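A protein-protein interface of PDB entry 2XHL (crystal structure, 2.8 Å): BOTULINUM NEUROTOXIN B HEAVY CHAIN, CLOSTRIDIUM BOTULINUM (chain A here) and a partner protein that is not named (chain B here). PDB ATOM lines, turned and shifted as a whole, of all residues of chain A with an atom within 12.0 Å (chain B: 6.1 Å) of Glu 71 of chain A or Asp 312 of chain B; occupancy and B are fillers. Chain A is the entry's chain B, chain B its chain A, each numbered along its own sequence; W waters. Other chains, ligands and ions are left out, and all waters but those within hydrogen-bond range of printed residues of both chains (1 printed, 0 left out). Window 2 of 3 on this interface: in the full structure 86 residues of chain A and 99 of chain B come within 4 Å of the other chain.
The side-chain amide oxygen (OD1) of Asn 139 of chain B sits at hydrogen-bond distance from the backbone NH (N) of Leu 73 of chain A (2.6 Å). N of Lys 152 of chain B sits close to OG of Ser 72 of chain A. O of Gly 153 of chain B sits at hydrogen-bond distance from N of Thr 70 of chain A (2.8 Å). N of Phe 155 of chain B sits at hydrogen-bond distance from O of Glu 68 of chain A (2.8 Å). The side-chain carboxylate of Asp 312 of chain B is in hydrogen-bond range of the side-chain hydroxyl of Thr 70 of chain A, at 2.9 Å.
OG1 of Thr 137 of chain B lies within hydrogen-bond range of O of Thr 131 of chain B, at 2.7 Å. The side-chain hydroxyl (OG1) of Thr 131 of chain B lies within hydrogen-bond range of the side-chain hydroxyl (OG) of Ser 311 of chain B (2.7 Å). The backbone carbonyl oxygen (O) of Asp 312 of chain B is in hydrogen-bond range of the side-chain sulfur (SG) of Cys 309 of chain B, at 3.4 Å. OD1 of Asp 312 of chain B is in hydrogen-bond range of N of Asn 314 of chain B (3.0 Å).
Gly 153 of chain B touches Glu 68 of chain A (O to O, 3.9 Å). Asn 69 of chain A touches Gly 153 of chain B. CG2 of Thr 70 of chain A touches CG2 of Thr 137 of chain B, 3.8 Å away. Thr 70 of chain A touches Ile 154 of chain B (CG2 to N, 3.9 Å). Thr 70 of chain A touches Phe 155 of chain B (CB to CZ, 3.6 Å). Thr 137 of chain B touches Glu 71 of chain A (CG2 to O, 3.6 Å). CA of Gly 153 of chain B touches O of Glu 71 of chain A, 3.6 Å away. O of Ser 311 of chain B touches CG of Glu 71 of chain A (3.4 Å). Ser 72 of chain A touches Gly 153 of chain B. ND2 of Asn 139 of chain B touches CE2 of Phe 76 of chain A, 3.6 Å away.
Of the printed residues of chain B, Asn 69 of chain A touches Gly 153 (3.7 Å). Of the printed residues of chain B, Thr 70 of chain A touches Thr 137, Gly 153, Ile 154, Phe 155 and Asp 312. Printed residues of chain B within 4 Å of Leu 73 of chain A: Thr 137 and Asn 139. Thr 137 of chain B touches just these residues of chain A: Thr 70 (3.8 Å), Glu 71 (3.6 Å) and Leu 73 (3.5 Å). Of the printed residues of chain A, Asn 139 of chain B touches Ser 72, Leu 73 and Phe 76. Printed residues of chain A within 4 Å of Lys 152 of chain B: Ser 72 (3.4 Å). Gly 153 of chain B touches just these residues of chain A: Glu 68 (3.9 Å), Asn 69 (3.7 Å), Thr 70 (2.8 Å), Glu 71 (3.6 Å) and Ser 72 (3.8 Å). Of the printed residues of chain A, Ile 154 of chain B touches Glu 68 (3.1 Å) and Thr 70 (3.9 Å). No residue of chain A comes within 4 Å of Cys 309 of chain B. No residue of chain A comes within 4 Å of Ile 310 of chain B. Asp 312 of chain B touches two residues of chain A. No residue of chain A comes within 4 Å of Pro 313 of chain B. No residue of chain A comes within 4 Å of Asn 314 of chain B. No residue of chain A comes within 4 Å of Ile 315 of chain B. The nearest residue of chain A that does not touch Asp 312 of chain B is Asn 69 of chain A (4.7 Å).
Of the 11 printed residues of chain A, 8 touch a printed residue of chain B. Of the 14 printed residues of chain B, 8 touch a printed residue of chain A. Hydrophobic or aromatic side chains of chain B within 4 Å of the printed part of chain A: Ile 154 and Phe 155. Among the printed residues, no Asp or Glu carboxylate lies within 4 Å of a Lys or Arg side-chain nitrogen of the other chain.
Water W1 lies within hydrogen-bond range of the backbone carbonyl oxygen of Phe 155 of chain B (2.6 Å) and the side-chain carboxylate of Glu 68 of chain A (2.7 Å).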
ATOM      1  N   PRO A  66      -6.211  -0.998 -24.444  1.00  0.00           N
ATOM      2  CA  PRO A  66      -7.424  -1.633 -24.972  1.00  0.00           C
ATOM      3  C   PRO A  66      -8.698  -0.958 -24.468  1.00  0.00           C
ATOM      4  O   PRO A  66      -8.652  -0.197 -23.496  1.00  0.00           O
ATOM      5  CB  PRO A  66      -7.341  -3.066 -24.428  1.00  0.00           C
ATOM      6  CG  PRO A  66      -5.922  -3.259 -24.036  1.00  0.00           C
ATOM      7  CD  PRO A  66      -5.453  -1.920 -23.579  1.00  0.00           C
ATOM      8  N   SER A  67      -9.820  -1.235 -25.129  1.00  0.00           N
ATOM      9  CA  SER A  67     -11.106  -0.667 -24.737  1.00  0.00           C
ATOM     10  C   SER A  67     -11.558  -1.212 -23.385  1.00  0.00           C
ATOM     11  O   SER A  67     -11.310  -2.374 -23.057  1.00  0.00           O
ATOM     12  CB  SER A  67     -12.167  -0.924 -25.807  1.00  0.00           C
ATOM     13  OG  SER A  67     -12.473  -2.302 -25.908  1.00  0.00           O
ATOM     14  N   GLU A  68     -12.220  -0.360 -22.608  1.00  0.00           N
ATOM     15  CA  GLU A  68     -12.640  -0.696 -21.251  1.00  0.00           C
ATOM     16  C   GLU A  68     -13.888  -1.582 -21.192  1.00  0.00           C
ATOM     17  O   GLU A  68     -14.135  -2.230 -20.178  1.00  0.00           O
ATOM     18  CB  GLU A  68     -12.853   0.579 -20.429  1.00  0.00           C
ATOM     19  CG  GLU A  68     -13.890   1.543 -21.005  1.00  0.00           C
ATOM     20  CD  GLU A  68     -13.962   2.862 -20.255  1.00  0.00           C
ATOM     21  OE1 GLU A  68     -13.070   3.137 -19.421  1.00  0.00           O
ATOM     22  OE2 GLU A  68     -14.914   3.630 -20.506  1.00  0.00           O
ATOM     23  N   ASN A  69     -14.659  -1.609 -22.277  1.00  0.00           N
ATOM     24  CA  ASN A  69     -15.920  -2.352 -22.327  1.00  0.00           C
ATOM     25  C   ASN A  69     -15.732  -3.865 -22.284  1.00  0.00           C
ATOM     26  O   ASN A  69     -14.948  -4.423 -23.051  1.00  0.00           O
ATOM     27  CB  ASN A  69     -16.725  -1.964 -23.571  1.00  0.00           C
ATOM     28  CG  ASN A  69     -17.000  -0.473 -23.653  1.00  0.00           C
ATOM     29  OD1 ASN A  69     -17.397   0.159 -22.671  1.00  0.00           O
ATOM     30  ND2 ASN A  69     -16.793   0.096 -24.838  1.00  0.00           N
ATOM     31  N   THR A  70     -16.457  -4.521 -21.380  1.00  0.00           N
ATOM     32  CA  THR A  70     -16.398  -5.977 -21.235  1.00  0.00           C
ATOM     33  C   THR A  70     -17.736  -6.559 -20.750  1.00  0.00           C
ATOM     34  O   THR A  70     -18.723  -5.832 -20.607  1.00  0.00           O
ATOM     35  CB  THR A  70     -15.214  -6.412 -20.317  1.00  0.00           C
ATOM     36  OG1 THR A  70     -15.022  -7.831 -20.400  1.00  0.00           O
ATOM     37  CG2 THR A  70     -15.449  -6.007 -18.863  1.00  0.00           C
ATOM     38  N   GLU A  71     -17.764  -7.872 -20.522  1.00  0.00           N
ATOM     39  CA  GLU A  71     -18.943  -8.556 -19.992  1.00  0.00           C
ATOM     40  C   GLU A  71     -19.155  -8.201 -18.525  1.00  0.00           C
ATOM     41  O   GLU A  71     -18.198  -7.900 -17.809  1.00  0.00           O
ATOM     42  CB  GLU A  71     -18.810 -10.075 -20.156  1.00  0.00           C
ATOM     43  CG  GLU A  71     -18.834 -10.561 -21.604  1.00  0.00           C
ATOM     44  CD  GLU A  71     -20.203 -10.438 -22.252  1.00  0.00           C
ATOM     45  OE1 GLU A  71     -20.380  -9.538 -23.099  1.00  0.00           O
ATOM     46  OE2 GLU A  71     -21.103 -11.235 -21.911  1.00  0.00           O
ATOM     47  N   SER A  72     -20.413  -8.238 -18.093  1.00  0.00           N
ATOM     48  CA  SER A  72     -20.790  -7.891 -16.723  1.00  0.00           C
ATOM     49  C   SER A  72     -20.216  -8.869 -15.705  1.00  0.00           C
ATOM     50  O   SER A  72     -19.983 -10.038 -16.016  1.00  0.00           O
ATOM     51  CB  SER A  72     -22.313  -7.845 -16.584  1.00  0.00           C
ATOM     52  OG  SER A  72     -22.882  -6.927 -17.499  1.00  0.00           O
ATOM     53  N   LEU A  73     -19.986  -8.373 -14.493  1.00  0.00           N
ATOM     54  CA  LEU A  73     -19.488  -9.188 -13.392  1.00  0.00           C
ATOM     55  C   LEU A  73     -20.644  -9.923 -12.717  1.00  0.00           C
ATOM     56  O   LEU A  73     -21.657  -9.312 -12.368  1.00  0.00           O
ATOM     57  CB  LEU A  73     -18.742  -8.308 -12.383  1.00  0.00           C
ATOM     58  CG  LEU A  73     -18.181  -8.921 -11.095  1.00  0.00           C
ATOM     59  CD1 LEU A  73     -16.987  -9.820 -11.378  1.00  0.00           C
ATOM     60  CD2 LEU A  73     -17.806  -7.827 -10.111  1.00  0.00           C
ATOM     61  N   THR A  74     -20.491 -11.233 -12.544  1.00  0.00           N
ATOM     62  CA  THR A  74     -21.513 -12.061 -11.898  1.00  0.00           C
ATOM     63  C   THR A  74     -20.996 -12.715 -10.615  1.00  0.00           C
ATOM     64  O   THR A  74     -21.768 -12.983  -9.691  1.00  0.00           O
ATOM     65  CB  THR A  74     -22.072 -13.149 -12.848  1.00  0.00           C
ATOM     66  OG1 THR A  74     -20.997 -13.943 -13.364  1.00  0.00           O
ATOM     67  CG2 THR A  74     -22.837 -12.518 -14.005  1.00  0.00           C
ATOM     68  N   ASP A  75     -19.691 -12.974 -10.567  1.00  0.00           N
ATOM     69  CA  ASP A  75     -19.061 -13.542  -9.381  1.00  0.00           C
ATOM     70  C   ASP A  75     -18.642 -12.419  -8.439  1.00  0.00           C
ATOM     71  O   ASP A  75     -17.604 -11.777  -8.633  1.00  0.00           O
ATOM     72  CB  ASP A  75     -17.858 -14.412  -9.769  1.00  0.00           C
ATOM     73  CG  ASP A  75     -17.383 -15.309  -8.631  1.00  0.00           C
ATOM     74  OD1 ASP A  75     -18.124 -15.483  -7.637  1.00  0.00           O
ATOM     75  OD2 ASP A  75     -16.260 -15.849  -8.738  1.00  0.00           O
ATOM     76  N   PHE A  76     -19.464 -12.180  -7.421  1.00  0.00           N
ATOM     77  CA  PHE A  76     -19.241 -11.076  -6.495  1.00  0.00           C
ATOM     78  C   PHE A  76     -18.467 -11.497  -5.246  1.00  0.00           C
ATOM     79  O   PHE A  76     -18.452 -10.772  -4.249  1.00  0.00           O
ATOM     80  CB  PHE A  76     -20.574 -10.419  -6.107  1.00  0.00           C
ATOM     81  CG  PHE A  76     -21.310  -9.799  -7.264  1.00  0.00           C
ATOM     82  CD1 PHE A  76     -22.476 -10.382  -7.751  1.00  0.00           C
ATOM     83  CD2 PHE A  76     -20.839  -8.637  -7.868  1.00  0.00           C
ATOM     84  CE1 PHE A  76     -23.163  -9.817  -8.821  1.00  0.00           C
ATOM     85  CE2 PHE A  76     -21.519  -8.063  -8.941  1.00  0.00           C
ATOM     86  CZ  PHE A  76     -22.685  -8.655  -9.417  1.00  0.00           C
ATOM     87  N   THR B 131     -12.208 -12.601 -16.646  1.00  0.00           N
ATOM     88  CA  THR B 131     -12.548 -11.231 -16.293  1.00  0.00           C
ATOM     89  C   THR B 131     -13.561 -11.197 -15.153  1.00  0.00           C
ATOM     90  O   THR B 131     -13.635 -10.212 -14.414  1.00  0.00           O
ATOM     91  CB  THR B 131     -13.108 -10.462 -17.504  1.00  0.00           C
ATOM     92  OG1 THR B 131     -14.369 -11.023 -17.888  1.00  0.00           O
ATOM     93  CG2 THR B 131     -12.143 -10.531 -18.683  1.00  0.00           C
ATOM     94  N   THR B 137     -13.085  -6.715 -12.933  1.00  0.00           N
ATOM     95  CA  THR B 137     -14.254  -6.076 -13.544  1.00  0.00           C
ATOM     96  C   THR B 137     -15.166  -5.372 -12.531  1.00  0.00           C
ATOM     97  O   THR B 137     -15.294  -5.798 -11.378  1.00  0.00           O
ATOM     98  CB  THR B 137     -15.072  -7.084 -14.397  1.00  0.00           C
ATOM     99  OG1 THR B 137     -14.199  -7.759 -15.313  1.00  0.00           O
ATOM    100  CG2 THR B 137     -16.173  -6.377 -15.189  1.00  0.00           C
ATOM    101  N   ASN B 139     -19.160  -3.312 -12.500  1.00  0.00           N
ATOM    102  CA  ASN B 139     -20.390  -3.125 -13.275  1.00  0.00           C
ATOM    103  C   ASN B 139     -20.862  -1.680 -13.353  1.00  0.00           C
ATOM    104  O   ASN B 139     -20.779  -0.936 -12.378  1.00  0.00           O
ATOM    105  CB  ASN B 139     -21.522  -4.003 -12.730  1.00  0.00           C
ATOM    106  CG  ASN B 139     -21.286  -5.484 -12.963  1.00  0.00           C
ATOM    107  OD1 ASN B 139     -20.642  -5.882 -13.933  1.00  0.00           O
ATOM    108  ND2 ASN B 139     -21.822  -6.311 -12.073  1.00  0.00           N
ATOM    109  N   LYS B 152     -23.561  -3.551 -17.580  1.00  0.00           N
ATOM    110  CA  LYS B 152     -22.441  -3.715 -18.497  1.00  0.00           C
ATOM    111  C   LYS B 152     -21.133  -3.634 -17.718  1.00  0.00           C
ATOM    112  O   LYS B 152     -21.042  -2.910 -16.724  1.00  0.00           O
ATOM    113  CB  LYS B 152     -22.479  -2.640 -19.584  1.00  0.00           C
ATOM    114  CG  LYS B 152     -21.995  -3.108 -20.948  1.00  0.00           C
ATOM    115  CD  LYS B 152     -23.099  -3.831 -21.706  1.00  0.00           C
ATOM    116  CE  LYS B 152     -22.575  -4.466 -22.982  1.00  0.00           C
ATOM    117  NZ  LYS B 152     -23.619  -5.302 -23.636  1.00  0.00           N
ATOM    118  N   GLY B 153     -20.127  -4.380 -18.165  1.00  0.00           N
ATOM    119  CA  GLY B 153     -18.829  -4.405 -17.491  1.00  0.00           C
ATOM    120  C   GLY B 153     -17.807  -3.444 -18.076  1.00  0.00           C
ATOM    121  O   GLY B 153     -17.757  -3.241 -19.290  1.00  0.00           O
ATOM    122  N   ILE B 154     -17.002  -2.840 -17.204  1.00  0.00           N
ATOM    123  CA  ILE B 154     -15.864  -2.021 -17.628  1.00  0.00           C
ATOM    124  C   ILE B 154     -14.596  -2.377 -16.848  1.00  0.00           C
ATOM    125  O   ILE B 154     -14.668  -2.782 -15.684  1.00  0.00           O
ATOM    126  CB  ILE B 154     -16.129  -0.489 -17.511  1.00  0.00           C
ATOM    127  CG1 ILE B 154     -16.537  -0.102 -16.088  1.00  0.00           C
ATOM    128  CG2 ILE B 154     -17.164  -0.024 -18.529  1.00  0.00           C
ATOM    129  CD1 ILE B 154     -16.138   1.301 -15.699  1.00  0.00           C
ATOM    130  N   PHE B 155     -13.443  -2.241 -17.502  1.00  0.00           N
ATOM    131  CA  PHE B 155     -12.149  -2.381 -16.838  1.00  0.00           C
ATOM    132  C   PHE B 155     -11.756  -1.062 -16.189  1.00  0.00           C
ATOM    133  O   PHE B 155     -11.899   0.005 -16.791  1.00  0.00           O
ATOM    134  CB  PHE B 155     -11.057  -2.805 -17.821  1.00  0.00           C
ATOM    135  CG  PHE B 155     -11.276  -4.153 -18.433  1.00  0.00           C
ATOM    136  CD1 PHE B 155     -11.397  -4.289 -19.809  1.00  0.00           C
ATOM    137  CD2 PHE B 155     -11.357  -5.292 -17.636  1.00  0.00           C
ATOM    138  CE1 PHE B 155     -11.598  -5.540 -20.386  1.00  0.00           C
ATOM    139  CE2 PHE B 155     -11.563  -6.550 -18.203  1.00  0.00           C
ATOM    140  CZ  PHE B 155     -11.682  -6.673 -19.580  1.00  0.00           C
ATOM    141  N   CYS B 309     -10.339 -17.082 -23.400  1.00  0.00           N
ATOM    142  CA  CYS B 309     -10.997 -16.296 -22.368  1.00  0.00           C
ATOM    143  C   CYS B 309     -12.450 -16.752 -22.288  1.00  0.00           C
ATOM    144  O   CYS B 309     -13.225 -16.557 -23.228  1.00  0.00           O
ATOM    145  CB  CYS B 309     -10.910 -14.805 -22.685  1.00  0.00           C
ATOM    146  SG  CYS B 309     -11.700 -13.743 -21.464  1.00  0.00           S
ATOM    147  N   ILE B 310     -12.805 -17.374 -21.167  1.00  0.00           N
ATOM    148  CA  ILE B 310     -14.124 -17.987 -20.994  1.00  0.00           C
ATOM    149  C   ILE B 310     -15.241 -16.983 -20.702  1.00  0.00           C
ATOM    150  O   ILE B 310     -16.359 -17.129 -21.204  1.00  0.00           O
ATOM    151  CB  ILE B 310     -14.107 -19.084 -19.901  1.00  0.00           C
ATOM    152  CG1 ILE B 310     -13.383 -18.582 -18.637  1.00  0.00           C
ATOM    153  CG2 ILE B 310     -13.461 -20.361 -20.449  1.00  0.00           C
ATOM    154  CD1 ILE B 310     -13.737 -19.333 -17.356  1.00  0.00           C
ATOM    155  N   SER B 311     -14.926 -15.969 -19.899  1.00  0.00           N
ATOM    156  CA  SER B 311     -15.913 -14.998 -19.427  1.00  0.00           C
ATOM    157  C   SER B 311     -16.345 -13.994 -20.495  1.00  0.00           C
ATOM    158  O   SER B 311     -17.473 -13.494 -20.459  1.00  0.00           O
ATOM    159  CB  SER B 311     -15.386 -14.258 -18.192  1.00  0.00           C
ATOM    160  OG  SER B 311     -14.128 -13.659 -18.450  1.00  0.00           O
ATOM    161  N   ASP B 312     -15.447 -13.703 -21.436  1.00  0.00           N
ATOM    162  CA  ASP B 312     -15.723 -12.747 -22.508  1.00  0.00           C
ATOM    163  C   ASP B 312     -15.144 -13.238 -23.838  1.00  0.00           C
ATOM    164  O   ASP B 312     -13.926 -13.369 -23.972  1.00  0.00           O
ATOM    165  CB  ASP B 312     -15.162 -11.363 -22.143  1.00  0.00           C
ATOM    166  CG  ASP B 312     -15.565 -10.268 -23.138  1.00  0.00           C
ATOM    167  OD1 ASP B 312     -16.413 -10.514 -24.027  1.00  0.00           O
ATOM    168  OD2 ASP B 312     -15.029  -9.143 -23.018  1.00  0.00           O
ATOM    169  N   PRO B 313     -16.021 -13.520 -24.822  1.00  0.00           N
ATOM    170  CA  PRO B 313     -15.585 -13.956 -26.153  1.00  0.00           C
ATOM    171  C   PRO B 313     -15.018 -12.825 -27.019  1.00  0.00           C
ATOM    172  O   PRO B 313     -14.353 -13.097 -28.022  1.00  0.00           O
ATOM    173  CB  PRO B 313     -16.872 -14.509 -26.785  1.00  0.00           C
ATOM    174  CG  PRO B 313     -17.843 -14.674 -25.653  1.00  0.00           C
ATOM    175  CD  PRO B 313     -17.485 -13.599 -24.684  1.00  0.00           C
ATOM    176  N   ASN B 314     -15.277 -11.576 -26.634  1.00  0.00           N
ATOM    177  CA  ASN B 314     -14.819 -10.412 -27.400  1.00  0.00           C
ATOM    178  C   ASN B 314     -13.418  -9.926 -27.027  1.00  0.00           C
ATOM    179  O   ASN B 314     -12.935  -8.929 -27.569  1.00  0.00           O
ATOM    180  CB  ASN B 314     -15.830  -9.263 -27.290  1.00  0.00           C
ATOM    181  CG  ASN B 314     -17.123  -9.546 -28.038  1.00  0.00           C
ATOM    182  OD1 ASN B 314     -18.215  -9.395 -27.488  1.00  0.00           O
ATOM    183  ND2 ASN B 314     -17.007  -9.961 -29.297  1.00  0.00           N
ATOM    184  N   ILE B 315     -12.776 -10.632 -26.098  1.00  0.00           N
ATOM    185  CA  ILE B 315     -11.397 -10.346 -25.715  1.00  0.00           C
ATOM    186  C   ILE B 315     -10.447 -10.954 -26.750  1.00  0.00           C
ATOM    187  O   ILE B 315     -10.433 -12.171 -26.954  1.00  0.00           O
ATOM    188  CB  ILE B 315     -11.068 -10.897 -24.288  1.00  0.00           C
ATOM    189  CG1 ILE B 315     -11.884 -10.178 -23.204  1.00  0.00           C
ATOM    190  CG2 ILE B 315      -9.566 -10.827 -23.986  1.00  0.00           C
ATOM    191  CD1 ILE B 315     -11.557  -8.699 -23.004  1.00  0.00           C
HETATM  192  O   HOH W   1     -12.224   2.587 -16.957  1.00  0.00           O
